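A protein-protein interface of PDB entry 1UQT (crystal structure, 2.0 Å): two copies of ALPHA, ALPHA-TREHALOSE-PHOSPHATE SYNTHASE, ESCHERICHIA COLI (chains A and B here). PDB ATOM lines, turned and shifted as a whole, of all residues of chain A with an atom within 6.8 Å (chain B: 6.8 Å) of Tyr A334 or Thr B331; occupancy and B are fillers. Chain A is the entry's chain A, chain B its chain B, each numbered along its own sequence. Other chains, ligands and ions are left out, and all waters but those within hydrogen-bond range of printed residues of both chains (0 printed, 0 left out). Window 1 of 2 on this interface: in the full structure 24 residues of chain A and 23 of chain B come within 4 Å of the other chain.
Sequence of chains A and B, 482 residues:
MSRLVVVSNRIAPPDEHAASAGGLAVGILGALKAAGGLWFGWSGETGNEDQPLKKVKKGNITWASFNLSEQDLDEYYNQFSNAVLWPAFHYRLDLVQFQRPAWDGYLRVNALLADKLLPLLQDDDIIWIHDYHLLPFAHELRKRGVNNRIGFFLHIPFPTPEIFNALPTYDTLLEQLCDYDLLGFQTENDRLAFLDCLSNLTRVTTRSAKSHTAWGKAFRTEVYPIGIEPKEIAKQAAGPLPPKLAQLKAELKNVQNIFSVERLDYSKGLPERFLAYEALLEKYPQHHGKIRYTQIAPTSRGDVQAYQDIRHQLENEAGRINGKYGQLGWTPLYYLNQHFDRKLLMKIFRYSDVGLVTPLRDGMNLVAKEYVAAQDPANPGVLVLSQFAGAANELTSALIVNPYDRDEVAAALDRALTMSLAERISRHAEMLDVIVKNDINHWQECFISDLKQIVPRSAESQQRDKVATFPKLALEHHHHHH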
ATOM      1  N   PHE A 274      -8.285 -25.160 -22.891  1.00  0.00           N
ATOM      2  CA  PHE A 274      -7.402 -24.507 -23.847  1.00  0.00           C
ATOM      3  C   PHE A 274      -8.241 -23.710 -24.833  1.00  0.00           C
ATOM      4  O   PHE A 274      -7.854 -22.643 -25.226  1.00  0.00           O
ATOM      5  CB  PHE A 274      -6.581 -25.523 -24.571  1.00  0.00           C
ATOM      6  CG  PHE A 274      -5.376 -25.989 -23.803  1.00  0.00           C
ATOM      7  CD1 PHE A 274      -5.337 -25.956 -22.421  1.00  0.00           C
ATOM      8  CD2 PHE A 274      -4.280 -26.494 -24.482  1.00  0.00           C
ATOM      9  CE1 PHE A 274      -4.198 -26.391 -21.747  1.00  0.00           C
ATOM     10  CE2 PHE A 274      -3.162 -26.931 -23.795  1.00  0.00           C
ATOM     11  CZ  PHE A 274      -3.132 -26.872 -22.440  1.00  0.00           C
ATOM     12  N   TYR A 277      -9.252 -20.540 -23.254  1.00  0.00           N
ATOM     13  CA  TYR A 277      -8.169 -19.554 -23.248  1.00  0.00           C
ATOM     14  C   TYR A 277      -8.046 -18.921 -24.626  1.00  0.00           C
ATOM     15  O   TYR A 277      -7.810 -17.722 -24.766  1.00  0.00           O
ATOM     16  CB  TYR A 277      -6.835 -20.204 -22.851  1.00  0.00           C
ATOM     17  CG  TYR A 277      -5.695 -19.258 -22.692  1.00  0.00           C
ATOM     18  CD1 TYR A 277      -5.763 -18.188 -21.802  1.00  0.00           C
ATOM     19  CD2 TYR A 277      -4.518 -19.430 -23.408  1.00  0.00           C
ATOM     20  CE1 TYR A 277      -4.702 -17.319 -21.630  1.00  0.00           C
ATOM     21  CE2 TYR A 277      -3.437 -18.584 -23.224  1.00  0.00           C
ATOM     22  CZ  TYR A 277      -3.540 -17.521 -22.348  1.00  0.00           C
ATOM     23  OH  TYR A 277      -2.469 -16.684 -22.186  1.00  0.00           O
ATOM     24  N   ARG A 292      -0.293 -14.825 -18.930  1.00  0.00           N
ATOM     25  CA  ARG A 292       0.245 -16.135 -19.212  1.00  0.00           C
ATOM     26  C   ARG A 292      -0.622 -17.183 -18.549  1.00  0.00           C
ATOM     27  O   ARG A 292      -1.050 -16.978 -17.406  1.00  0.00           O
ATOM     28  CB  ARG A 292       1.653 -16.225 -18.656  1.00  0.00           C
ATOM     29  CG  ARG A 292       2.548 -17.042 -19.489  1.00  0.00           C
ATOM     30  CD  ARG A 292       3.915 -16.375 -19.664  1.00  0.00           C
ATOM     31  NE  ARG A 292       4.796 -17.003 -18.716  1.00  0.00           N
ATOM     32  CZ  ARG A 292       6.059 -16.692 -18.544  1.00  0.00           C
ATOM     33  NH1 ARG A 292       6.645 -15.713 -19.237  1.00  0.00           N
ATOM     34  NH2 ARG A 292       6.736 -17.384 -17.646  1.00  0.00           N
ATOM     35  N   TYR A 293      -0.911 -18.263 -19.288  1.00  0.00           N
ATOM     36  CA  TYR A 293      -1.652 -19.388 -18.793  1.00  0.00           C
ATOM     37  C   TYR A 293      -0.662 -20.547 -18.788  1.00  0.00           C
ATOM     38  O   TYR A 293      -0.061 -20.872 -19.826  1.00  0.00           O
ATOM     39  CB  TYR A 293      -2.891 -19.654 -19.680  1.00  0.00           C
ATOM     40  CG  TYR A 293      -3.601 -21.017 -19.479  1.00  0.00           C
ATOM     41  CD1 TYR A 293      -3.640 -21.655 -18.226  1.00  0.00           C
ATOM     42  CD2 TYR A 293      -4.198 -21.665 -20.557  1.00  0.00           C
ATOM     43  CE1 TYR A 293      -4.251 -22.881 -18.068  1.00  0.00           C
ATOM     44  CE2 TYR A 293      -4.817 -22.880 -20.412  1.00  0.00           C
ATOM     45  CZ  TYR A 293      -4.840 -23.492 -19.173  1.00  0.00           C
ATOM     46  OH  TYR A 293      -5.443 -24.707 -19.066  1.00  0.00           O
ATOM     47  N   THR A 294      -0.431 -21.121 -17.611  1.00  0.00           N
ATOM     48  CA  THR A 294       0.477 -22.280 -17.472  1.00  0.00           C
ATOM     49  C   THR A 294      -0.397 -23.442 -17.048  1.00  0.00           C
ATOM     50  O   THR A 294      -1.169 -23.318 -16.087  1.00  0.00           O
ATOM     51  CB  THR A 294       1.580 -22.022 -16.420  1.00  0.00           C
ATOM     52  OG1 THR A 294       2.380 -20.896 -16.787  1.00  0.00           O
ATOM     53  CG2 THR A 294       2.590 -23.188 -16.342  1.00  0.00           C
ATOM     54  N   GLN A 295      -0.294 -24.549 -17.790  1.00  0.00           N
ATOM     55  CA  GLN A 295      -0.996 -25.772 -17.485  1.00  0.00           C
ATOM     56  C   GLN A 295       0.031 -26.824 -17.184  1.00  0.00           C
ATOM     57  O   GLN A 295       0.833 -27.177 -18.054  1.00  0.00           O
ATOM     58  CB  GLN A 295      -1.823 -26.225 -18.670  1.00  0.00           C
ATOM     59  CG  GLN A 295      -2.464 -27.612 -18.481  1.00  0.00           C
ATOM     60  CD  GLN A 295      -3.566 -27.592 -17.478  1.00  0.00           C
ATOM     61  OE1 GLN A 295      -4.531 -26.852 -17.660  1.00  0.00           O
ATOM     62  NE2 GLN A 295      -3.428 -28.370 -16.382  1.00  0.00           N
ATOM     63  N   ILE A 296       0.040 -27.277 -15.934  1.00  0.00           N
ATOM     64  CA  ILE A 296       0.867 -28.391 -15.483  1.00  0.00           C
ATOM     65  C   ILE A 296      -0.003 -29.647 -15.539  1.00  0.00           C
ATOM     66  O   ILE A 296      -1.105 -29.677 -15.017  1.00  0.00           O
ATOM     67  CB  ILE A 296       1.425 -28.118 -14.081  1.00  0.00           C
ATOM     68  CG1 ILE A 296       2.362 -26.921 -14.160  1.00  0.00           C
ATOM     69  CG2 ILE A 296       2.121 -29.360 -13.552  1.00  0.00           C
ATOM     70  CD1 ILE A 296       3.046 -26.531 -12.859  1.00  0.00           C
ATOM     71  N   ALA A 318      -2.024 -27.003 -27.729  1.00  0.00           N
ATOM     72  CA  ALA A 318      -0.966 -26.108 -27.275  1.00  0.00           C
ATOM     73  C   ALA A 318      -0.229 -25.543 -28.446  1.00  0.00           C
ATOM     74  O   ALA A 318       0.025 -24.358 -28.499  1.00  0.00           O
ATOM     75  CB  ALA A 318       0.050 -26.819 -26.348  1.00  0.00           C
ATOM     76  N   ASN A 322      -0.617 -21.498 -29.508  1.00  0.00           N
ATOM     77  CA  ASN A 322       0.632 -20.740 -29.542  1.00  0.00           C
ATOM     78  C   ASN A 322       1.019 -20.404 -30.969  1.00  0.00           C
ATOM     79  O   ASN A 322       1.600 -19.360 -31.235  1.00  0.00           O
ATOM     80  CB  ASN A 322       1.789 -21.507 -28.857  1.00  0.00           C
ATOM     81  CG  ASN A 322       1.655 -21.501 -27.356  1.00  0.00           C
ATOM     82  OD1 ASN A 322       1.072 -20.548 -26.794  1.00  0.00           O
ATOM     83  ND2 ASN A 322       2.175 -22.556 -26.679  1.00  0.00           N
ATOM     84  N   TRP A 330       6.512 -13.546 -26.962  1.00  0.00           N
ATOM     85  CA  TRP A 330       5.382 -13.872 -26.091  1.00  0.00           C
ATOM     86  C   TRP A 330       4.711 -15.190 -26.461  1.00  0.00           C
ATOM     87  O   TRP A 330       4.056 -15.294 -27.488  1.00  0.00           O
ATOM     88  CB  TRP A 330       4.340 -12.760 -26.105  1.00  0.00           C
ATOM     89  CG  TRP A 330       3.221 -13.004 -25.150  1.00  0.00           C
ATOM     90  CD1 TRP A 330       3.319 -13.159 -23.789  1.00  0.00           C
ATOM     91  CD2 TRP A 330       1.828 -13.128 -25.467  1.00  0.00           C
ATOM     92  NE1 TRP A 330       2.075 -13.375 -23.254  1.00  0.00           N
ATOM     93  CE2 TRP A 330       1.140 -13.353 -24.258  1.00  0.00           C
ATOM     94  CE3 TRP A 330       1.087 -13.051 -26.654  1.00  0.00           C
ATOM     95  CZ2 TRP A 330      -0.259 -13.516 -24.196  1.00  0.00           C
ATOM     96  CZ3 TRP A 330      -0.303 -13.213 -26.590  1.00  0.00           C
ATOM     97  CH2 TRP A 330      -0.951 -13.448 -25.363  1.00  0.00           C
ATOM     98  N   THR A 331       4.878 -16.189 -25.592  1.00  0.00           N
ATOM     99  CA  THR A 331       4.127 -17.430 -25.663  1.00  0.00           C
ATOM    100  C   THR A 331       2.931 -17.327 -24.719  1.00  0.00           C
ATOM    101  O   THR A 331       3.116 -17.201 -23.505  1.00  0.00           O
ATOM    102  CB  THR A 331       5.021 -18.607 -25.264  1.00  0.00           C
ATOM    103  OG1 THR A 331       6.110 -18.719 -26.196  1.00  0.00           O
ATOM    104  CG2 THR A 331       4.275 -19.928 -25.426  1.00  0.00           C
ATOM    105  N   PRO A 332       1.716 -17.358 -25.265  1.00  0.00           N
ATOM    106  CA  PRO A 332       0.503 -17.298 -24.444  1.00  0.00           C
ATOM    107  C   PRO A 332       0.306 -18.481 -23.510  1.00  0.00           C
ATOM    108  O   PRO A 332      -0.160 -18.263 -22.402  1.00  0.00           O
ATOM    109  CB  PRO A 332      -0.641 -17.283 -25.467  1.00  0.00           C
ATOM    110  CG  PRO A 332      -0.025 -17.114 -26.786  1.00  0.00           C
ATOM    111  CD  PRO A 332       1.415 -17.342 -26.707  1.00  0.00           C
ATOM    112  N   LEU A 333       0.612 -19.691 -23.979  1.00  0.00           N
ATOM    113  CA  LEU A 333       0.272 -20.918 -23.277  1.00  0.00           C
ATOM    114  C   LEU A 333       1.543 -21.713 -23.032  1.00  0.00           C
ATOM    115  O   LEU A 333       2.224 -22.078 -23.985  1.00  0.00           O
ATOM    116  CB  LEU A 333      -0.706 -21.744 -24.115  1.00  0.00           C
ATOM    117  CG  LEU A 333      -1.728 -22.571 -23.344  1.00  0.00           C
ATOM    118  CD1 LEU A 333      -2.843 -23.120 -24.204  1.00  0.00           C
ATOM    119  CD2 LEU A 333      -1.031 -23.688 -22.640  1.00  0.00           C
ATOM    120  N   TYR A 334       1.850 -21.950 -21.762  1.00  0.00           N
ATOM    121  CA  TYR A 334       2.963 -22.775 -21.319  1.00  0.00           C
ATOM    122  C   TYR A 334       2.359 -24.122 -20.872  1.00  0.00           C
ATOM    123  O   TYR A 334       1.626 -24.168 -19.895  1.00  0.00           O
ATOM    124  CB  TYR A 334       3.643 -22.107 -20.114  1.00  0.00           C
ATOM    125  CG  TYR A 334       4.606 -21.022 -20.459  1.00  0.00           C
ATOM    126  CD1 TYR A 334       4.212 -19.920 -21.225  1.00  0.00           C
ATOM    127  CD2 TYR A 334       5.920 -21.094 -20.054  1.00  0.00           C
ATOM    128  CE1 TYR A 334       5.114 -18.920 -21.573  1.00  0.00           C
ATOM    129  CE2 TYR A 334       6.811 -20.108 -20.396  1.00  0.00           C
ATOM    130  CZ  TYR A 334       6.401 -19.018 -21.152  1.00  0.00           C
ATOM    131  OH  TYR A 334       7.307 -18.058 -21.483  1.00  0.00           O
ATOM    132  N   TYR A 335       2.641 -25.195 -21.602  1.00  0.00           N
ATOM    133  CA  TYR A 335       2.156 -26.517 -21.276  1.00  0.00           C
ATOM    134  C   TYR A 335       3.317 -27.376 -20.842  1.00  0.00           C
ATOM    135  O   TYR A 335       4.266 -27.517 -21.557  1.00  0.00           O
ATOM    136  CB  TYR A 335       1.468 -27.113 -22.500  1.00  0.00           C
ATOM    137  CG  TYR A 335       1.300 -28.598 -22.501  1.00  0.00           C
ATOM    138  CD1 TYR A 335       0.465 -29.252 -21.583  1.00  0.00           C
ATOM    139  CD2 TYR A 335       1.976 -29.370 -23.432  1.00  0.00           C
ATOM    140  CE1 TYR A 335       0.309 -30.637 -21.635  1.00  0.00           C
ATOM    141  CE2 TYR A 335       1.831 -30.734 -23.475  1.00  0.00           C
ATOM    142  CZ  TYR A 335       1.017 -31.377 -22.577  1.00  0.00           C
ATOM    143  OH  TYR A 335       0.940 -32.766 -22.671  1.00  0.00           O
ATOM    144  N   LEU A 336       3.205 -27.967 -19.659  1.00  0.00           N
ATOM    145  CA  LEU A 336       4.275 -28.764 -19.068  1.00  0.00           C
ATOM    146  C   LEU A 336       3.685 -30.106 -18.671  1.00  0.00           C
ATOM    147  O   LEU A 336       2.844 -30.185 -17.775  1.00  0.00           O
ATOM    148  CB  LEU A 336       4.841 -28.063 -17.840  1.00  0.00           C
ATOM    149  CG  LEU A 336       5.371 -26.659 -18.104  1.00  0.00           C
ATOM    150  CD1 LEU A 336       5.816 -26.017 -16.825  1.00  0.00           C
ATOM    151  CD2 LEU A 336       6.535 -26.707 -19.106  1.00  0.00           C
ATOM    152  N   TYR B 277      16.097 -30.579 -32.960  1.00  0.00           N
ATOM    153  CA  TYR B 277      16.142 -29.698 -31.815  1.00  0.00           C
ATOM    154  C   TYR B 277      15.913 -30.496 -30.539  1.00  0.00           C
ATOM    155  O   TYR B 277      16.598 -30.294 -29.551  1.00  0.00           O
ATOM    156  CB  TYR B 277      15.081 -28.611 -31.932  1.00  0.00           C
ATOM    157  CG  TYR B 277      15.181 -27.579 -30.856  1.00  0.00           C
ATOM    158  CD1 TYR B 277      16.355 -26.870 -30.642  1.00  0.00           C
ATOM    159  CD2 TYR B 277      14.064 -27.260 -30.074  1.00  0.00           C
ATOM    160  CE1 TYR B 277      16.421 -25.931 -29.657  1.00  0.00           C
ATOM    161  CE2 TYR B 277      14.122 -26.307 -29.120  1.00  0.00           C
ATOM    162  CZ  TYR B 277      15.310 -25.652 -28.898  1.00  0.00           C
ATOM    163  OH  TYR B 277      15.341 -24.692 -27.929  1.00  0.00           O
ATOM    164  N   ILE B 291      19.026 -21.232 -24.718  1.00  0.00           N
ATOM    165  CA  ILE B 291      18.797 -21.158 -26.155  1.00  0.00           C
ATOM    166  C   ILE B 291      17.319 -21.199 -26.430  1.00  0.00           C
ATOM    167  O   ILE B 291      16.498 -21.543 -25.588  1.00  0.00           O
ATOM    168  CB  ILE B 291      19.460 -22.340 -26.917  1.00  0.00           C
ATOM    169  CG1 ILE B 291      18.712 -23.651 -26.625  1.00  0.00           C
ATOM    170  CG2 ILE B 291      20.958 -22.432 -26.572  1.00  0.00           C
ATOM    171  CD1 ILE B 291      19.259 -24.843 -27.313  1.00  0.00           C
ATOM    172  N   ARG B 292      16.993 -20.914 -27.667  1.00  0.00           N
ATOM    173  CA  ARG B 292      15.642 -21.059 -28.110  1.00  0.00           C
ATOM    174  C   ARG B 292      15.604 -21.234 -29.621  1.00  0.00           C
ATOM    175  O   ARG B 292      16.373 -20.625 -30.336  1.00  0.00           O
ATOM    176  CB  ARG B 292      14.894 -19.828 -27.673  1.00  0.00           C
ATOM    177  CG  ARG B 292      14.015 -19.285 -28.727  1.00  0.00           C
ATOM    178  CD  ARG B 292      12.608 -19.195 -28.366  1.00  0.00           C
ATOM    179  NE  ARG B 292      12.167 -17.814 -28.250  1.00  0.00           N
ATOM    180  CZ  ARG B 292      12.379 -17.020 -27.207  1.00  0.00           C
ATOM    181  NH1 ARG B 292      13.104 -17.432 -26.183  1.00  0.00           N
ATOM    182  NH2 ARG B 292      11.868 -15.791 -27.204  1.00  0.00           N
ATOM    183  N   TYR B 293      14.703 -22.079 -30.086  1.00  0.00           N
ATOM    184  CA  TYR B 293      14.492 -22.301 -31.510  1.00  0.00           C
ATOM    185  C   TYR B 293      13.131 -21.714 -31.864  1.00  0.00           C
ATOM    186  O   TYR B 293      12.148 -22.035 -31.237  1.00  0.00           O
ATOM    187  CB  TYR B 293      14.564 -23.802 -31.795  1.00  0.00           C
ATOM    188  CG  TYR B 293      14.075 -24.247 -33.156  1.00  0.00           C
ATOM    189  CD1 TYR B 293      14.305 -23.493 -34.299  1.00  0.00           C
ATOM    190  CD2 TYR B 293      13.384 -25.443 -33.289  1.00  0.00           C
ATOM    191  CE1 TYR B 293      13.846 -23.923 -35.540  1.00  0.00           C
ATOM    192  CE2 TYR B 293      12.920 -25.877 -34.520  1.00  0.00           C
ATOM    193  CZ  TYR B 293      13.162 -25.118 -35.641  1.00  0.00           C
ATOM    194  OH  TYR B 293      12.707 -25.563 -36.841  1.00  0.00           O
ATOM    195  N   ASN B 322       7.870 -28.908 -26.117  1.00  0.00           N
ATOM    196  CA  ASN B 322       7.734 -27.923 -25.055  1.00  0.00           C
ATOM    197  C   ASN B 322       7.216 -28.534 -23.779  1.00  0.00           C
ATOM    198  O   ASN B 322       7.683 -28.176 -22.729  1.00  0.00           O
ATOM    199  CB  ASN B 322       6.855 -26.735 -25.497  1.00  0.00           C
ATOM    200  CG  ASN B 322       7.608 -25.818 -26.465  1.00  0.00           C
ATOM    201  OD1 ASN B 322       8.842 -25.692 -26.363  1.00  0.00           O
ATOM    202  ND2 ASN B 322       6.890 -25.210 -27.427  1.00  0.00           N
ATOM    203  N   TYR B 325      10.428 -30.643 -22.317  1.00  0.00           N
ATOM    204  CA  TYR B 325      11.640 -29.885 -21.953  1.00  0.00           C
ATOM    205  C   TYR B 325      11.407 -28.499 -21.386  1.00  0.00           C
ATOM    206  O   TYR B 325      12.331 -27.869 -20.880  1.00  0.00           O
ATOM    207  CB  TYR B 325      12.574 -29.758 -23.160  1.00  0.00           C
ATOM    208  CG  TYR B 325      13.104 -31.086 -23.595  1.00  0.00           C
ATOM    209  CD1 TYR B 325      14.158 -31.700 -22.906  1.00  0.00           C
ATOM    210  CD2 TYR B 325      12.539 -31.755 -24.664  1.00  0.00           C
ATOM    211  CE1 TYR B 325      14.632 -32.943 -23.299  1.00  0.00           C
ATOM    212  CE2 TYR B 325      12.996 -32.991 -25.044  1.00  0.00           C
ATOM    213  CZ  TYR B 325      14.034 -33.587 -24.353  1.00  0.00           C
ATOM    214  OH  TYR B 325      14.477 -34.807 -24.770  1.00  0.00           O
ATOM    215  N   GLY B 326      10.183 -28.010 -21.463  1.00  0.00           N
ATOM    216  CA  GLY B 326       9.902 -26.673 -20.988  1.00  0.00           C
ATOM    217  C   GLY B 326       9.929 -26.573 -19.469  1.00  0.00           C
ATOM    218  O   GLY B 326       9.872 -27.584 -18.732  1.00  0.00           O
ATOM    219  N   GLN B 327      10.026 -25.323 -19.021  1.00  0.00           N
ATOM    220  CA  GLN B 327      10.049 -24.945 -17.609  1.00  0.00           C
ATOM    221  C   GLN B 327       9.102 -23.798 -17.418  1.00  0.00           C
ATOM    222  O   GLN B 327       8.631 -23.184 -18.388  1.00  0.00           O
ATOM    223  CB  GLN B 327      11.449 -24.504 -17.158  1.00  0.00           C
ATOM    224  CG  GLN B 327      12.551 -25.528 -17.459  1.00  0.00           C
ATOM    225  CD  GLN B 327      13.958 -24.983 -17.193  1.00  0.00           C
ATOM    226  OE1 GLN B 327      14.107 -23.883 -16.710  1.00  0.00           O
ATOM    227  NE2 GLN B 327      14.979 -25.750 -17.552  1.00  0.00           N
ATOM    228  N   LEU B 328       8.853 -23.469 -16.161  1.00  0.00           N
ATOM    229  CA  LEU B 328       7.944 -22.384 -15.872  1.00  0.00           C
ATOM    230  C   LEU B 328       8.396 -21.084 -16.496  1.00  0.00           C
ATOM    231  O   LEU B 328       7.561 -20.254 -16.832  1.00  0.00           O
ATOM    232  CB  LEU B 328       7.808 -22.173 -14.384  1.00  0.00           C
ATOM    233  CG  LEU B 328       7.117 -23.296 -13.653  1.00  0.00           C
ATOM    234  CD1 LEU B 328       7.348 -23.085 -12.175  1.00  0.00           C
ATOM    235  CD2 LEU B 328       5.614 -23.321 -14.036  1.00  0.00           C
ATOM    236  N   GLY B 329       9.706 -20.895 -16.622  1.00  0.00           N
ATOM    237  CA  GLY B 329      10.228 -19.648 -17.150  1.00  0.00           C
ATOM    238  C   GLY B 329      10.991 -19.785 -18.443  1.00  0.00           C
ATOM    239  O   GLY B 329      11.709 -18.866 -18.809  1.00  0.00           O
ATOM    240  N   TRP B 330      10.829 -20.912 -19.137  1.00  0.00           N
ATOM    241  CA  TRP B 330      11.522 -21.166 -20.382  1.00  0.00           C
ATOM    242  C   TRP B 330      10.747 -22.118 -21.330  1.00  0.00           C
ATOM    243  O   TRP B 330      10.472 -23.285 -20.998  1.00  0.00           O
ATOM    244  CB  TRP B 330      12.910 -21.714 -20.069  1.00  0.00           C
ATOM    245  CG  TRP B 330      13.693 -22.018 -21.288  1.00  0.00           C
ATOM    246  CD1 TRP B 330      14.098 -21.130 -22.236  1.00  0.00           C
ATOM    247  CD2 TRP B 330      14.173 -23.299 -21.706  1.00  0.00           C
ATOM    248  NE1 TRP B 330      14.815 -21.776 -23.201  1.00  0.00           N
ATOM    249  CE2 TRP B 330      14.847 -23.116 -22.920  1.00  0.00           C
ATOM    250  CE3 TRP B 330      14.078 -24.599 -21.183  1.00  0.00           C
ATOM    251  CZ2 TRP B 330      15.455 -24.156 -23.593  1.00  0.00           C
ATOM    252  CZ3 TRP B 330      14.675 -25.624 -21.845  1.00  0.00           C
ATOM    253  CH2 TRP B 330      15.358 -25.410 -23.038  1.00  0.00           C
ATOM    254  N   THR B 331      10.388 -21.597 -22.501  1.00  0.00           N
ATOM    255  CA  THR B 331       9.755 -22.366 -23.567  1.00  0.00           C
ATOM    256  C   THR B 331      10.847 -22.581 -24.609  1.00  0.00           C
ATOM    257  O   THR B 331      11.350 -21.600 -25.137  1.00  0.00           O
ATOM    258  CB  THR B 331       8.576 -21.555 -24.151  1.00  0.00           C
ATOM    259  OG1 THR B 331       7.549 -21.383 -23.156  1.00  0.00           O
ATOM    260  CG2 THR B 331       7.872 -22.318 -25.274  1.00  0.00           C
ATOM    261  N   PRO B 332      11.294 -23.822 -24.836  1.00  0.00           N
ATOM    262  CA  PRO B 332      12.376 -24.082 -25.790  1.00  0.00           C
ATOM    263  C   PRO B 332      12.093 -23.800 -27.267  1.00  0.00           C
ATOM    264  O   PRO B 332      13.044 -23.425 -28.014  1.00  0.00           O
ATOM    265  CB  PRO B 332      12.700 -25.579 -25.588  1.00  0.00           C
ATOM    266  CG  PRO B 332      11.821 -26.073 -24.539  1.00  0.00           C
ATOM    267  CD  PRO B 332      10.905 -25.028 -24.096  1.00  0.00           C
ATOM    268  N   LEU B 333      10.844 -23.987 -27.676  1.00  0.00           N
ATOM    269  CA  LEU B 333      10.451 -23.945 -29.091  1.00  0.00           C
ATOM    270  C   LEU B 333       9.306 -22.972 -29.318  1.00  0.00           C
ATOM    271  O   LEU B 333       8.240 -23.119 -28.733  1.00  0.00           O
ATOM    272  CB  LEU B 333      10.037 -25.338 -29.547  1.00  0.00           C
ATOM    273  CG  LEU B 333      10.009 -25.622 -31.048  1.00  0.00           C
ATOM    274  CD1 LEU B 333      10.186 -27.133 -31.305  1.00  0.00           C
ATOM    275  CD2 LEU B 333       8.690 -25.149 -31.644  1.00  0.00           C
ATOM    276  N   TYR B 334       9.519 -21.970 -30.155  1.00  0.00           N
ATOM    277  CA  TYR B 334       8.466 -21.024 -30.496  1.00  0.00           C
ATOM    278  C   TYR B 334       8.062 -21.423 -31.891  1.00  0.00           C
ATOM    279  O   TYR B 334       8.888 -21.367 -32.819  1.00  0.00           O
ATOM    280  CB  TYR B 334       8.982 -19.583 -30.489  1.00  0.00           C
ATOM    281  CG  TYR B 334       9.000 -18.938 -29.118  1.00  0.00           C
ATOM    282  CD1 TYR B 334       9.584 -19.597 -28.026  1.00  0.00           C
ATOM    283  CD2 TYR B 334       8.459 -17.686 -28.896  1.00  0.00           C
ATOM    284  CE1 TYR B 334       9.605 -19.036 -26.754  1.00  0.00           C
ATOM    285  CE2 TYR B 334       8.497 -17.108 -27.632  1.00  0.00           C
ATOM    286  CZ  TYR B 334       9.078 -17.806 -26.554  1.00  0.00           C
ATOM    287  OH  TYR B 334       9.136 -17.284 -25.277  1.00  0.00           O
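The backbone carbonyl oxygen (O) of Leu B328 is in hydrogen-bond range of the guanidinium group (NH2) of Arg A292 (3.1 Å).
The side-chain hydroxyl of Tyr B334 sits close to the side-chain hydroxyl of Thr A331, at 3.5 Å.
The guanidinium group of Arg A292 sits at hydrogen-bond distance from the side-chain hydroxyl of Tyr A334, 3.3 Å away.
The backbone NH of Tyr A334 lies within hydrogen-bond range of the backbone carbonyl oxygen of Tyr A293 (2.9 Å).
The backbone carbonyl oxygen of Tyr A334 lies within hydrogen-bond range of the backbone NH of Gln A295.
The backbone carbonyl oxygen (O) of Gln A295 lies within hydrogen-bond range of the backbone NH (N) of Leu A336 (3.0 Å).
N of Tyr B334 is in hydrogen-bond range of O of Tyr B293 (2.8 Å).
ND2 of Asn B322 is in hydrogen-bond range of O of Leu B333.
Among the printed residues, pairs that only touch across the chains: Thr A294 with Leu B328 (3.8 Å), Tyr A334 with Gln B327 (3.8 Å), Tyr A334 with Leu B328 (3.6 Å), Tyr A334 with Thr B331 (3.1 Å), Tyr A335 with Asn B322 (3.7 Å), Leu A336 with Gly B326 (3.4 Å), Leu A336 with Gln B327 (3.8 Å) and Leu A336 with Leu B328 (3.9 Å).
Of the printed residues of chain B, Tyr A334 touches Gln B327, Leu B328 and Thr B331.
Printed residues of chain A within 4 Å of Thr B331: Tyr A334.
Of the printed residues of chain A, Gly B326 touches Leu A336 (3.4 Å).
Of the printed residues of chain B, Tyr A335 touches Asn B322.
Printed residues of chain B within 4 Å of Thr A294: Leu B328 (3.8 Å).
Of the printed residues of chain B, Leu A336 touches Gly B326 (3.4 Å), Gln B327 (3.8 Å) and Leu B328 (3.9 Å).
Gly B329 touches none of the printed residues of chain A.
Trp A330 touches none of the printed residues of chain B.
The nearest printed residue of chain B that does not touch Tyr A334 is Tyr B334 (4.3 Å).
The nearest residue of chain A that does not touch Thr B331 is Thr A331 (4.1 Å).
Hydrophobic or aromatic side chains of chain A within 4 Å of the printed part of chain B: Tyr A334 and Leu A336.
Of the 15 printed residues of chain B, 6 touch a printed residue of chain A.
Hydrophobic or aromatic side chains of chain B that line the printed part of chain A: Leu B328 and Tyr B334.
Thr A331 touches Tyr B334, and with the chains exchanged Tyr A334 touches Thr B331.
Of the 10 pairs that touch across the chains among the printed residues, 2 have their exchanged pair printed and touching as well.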
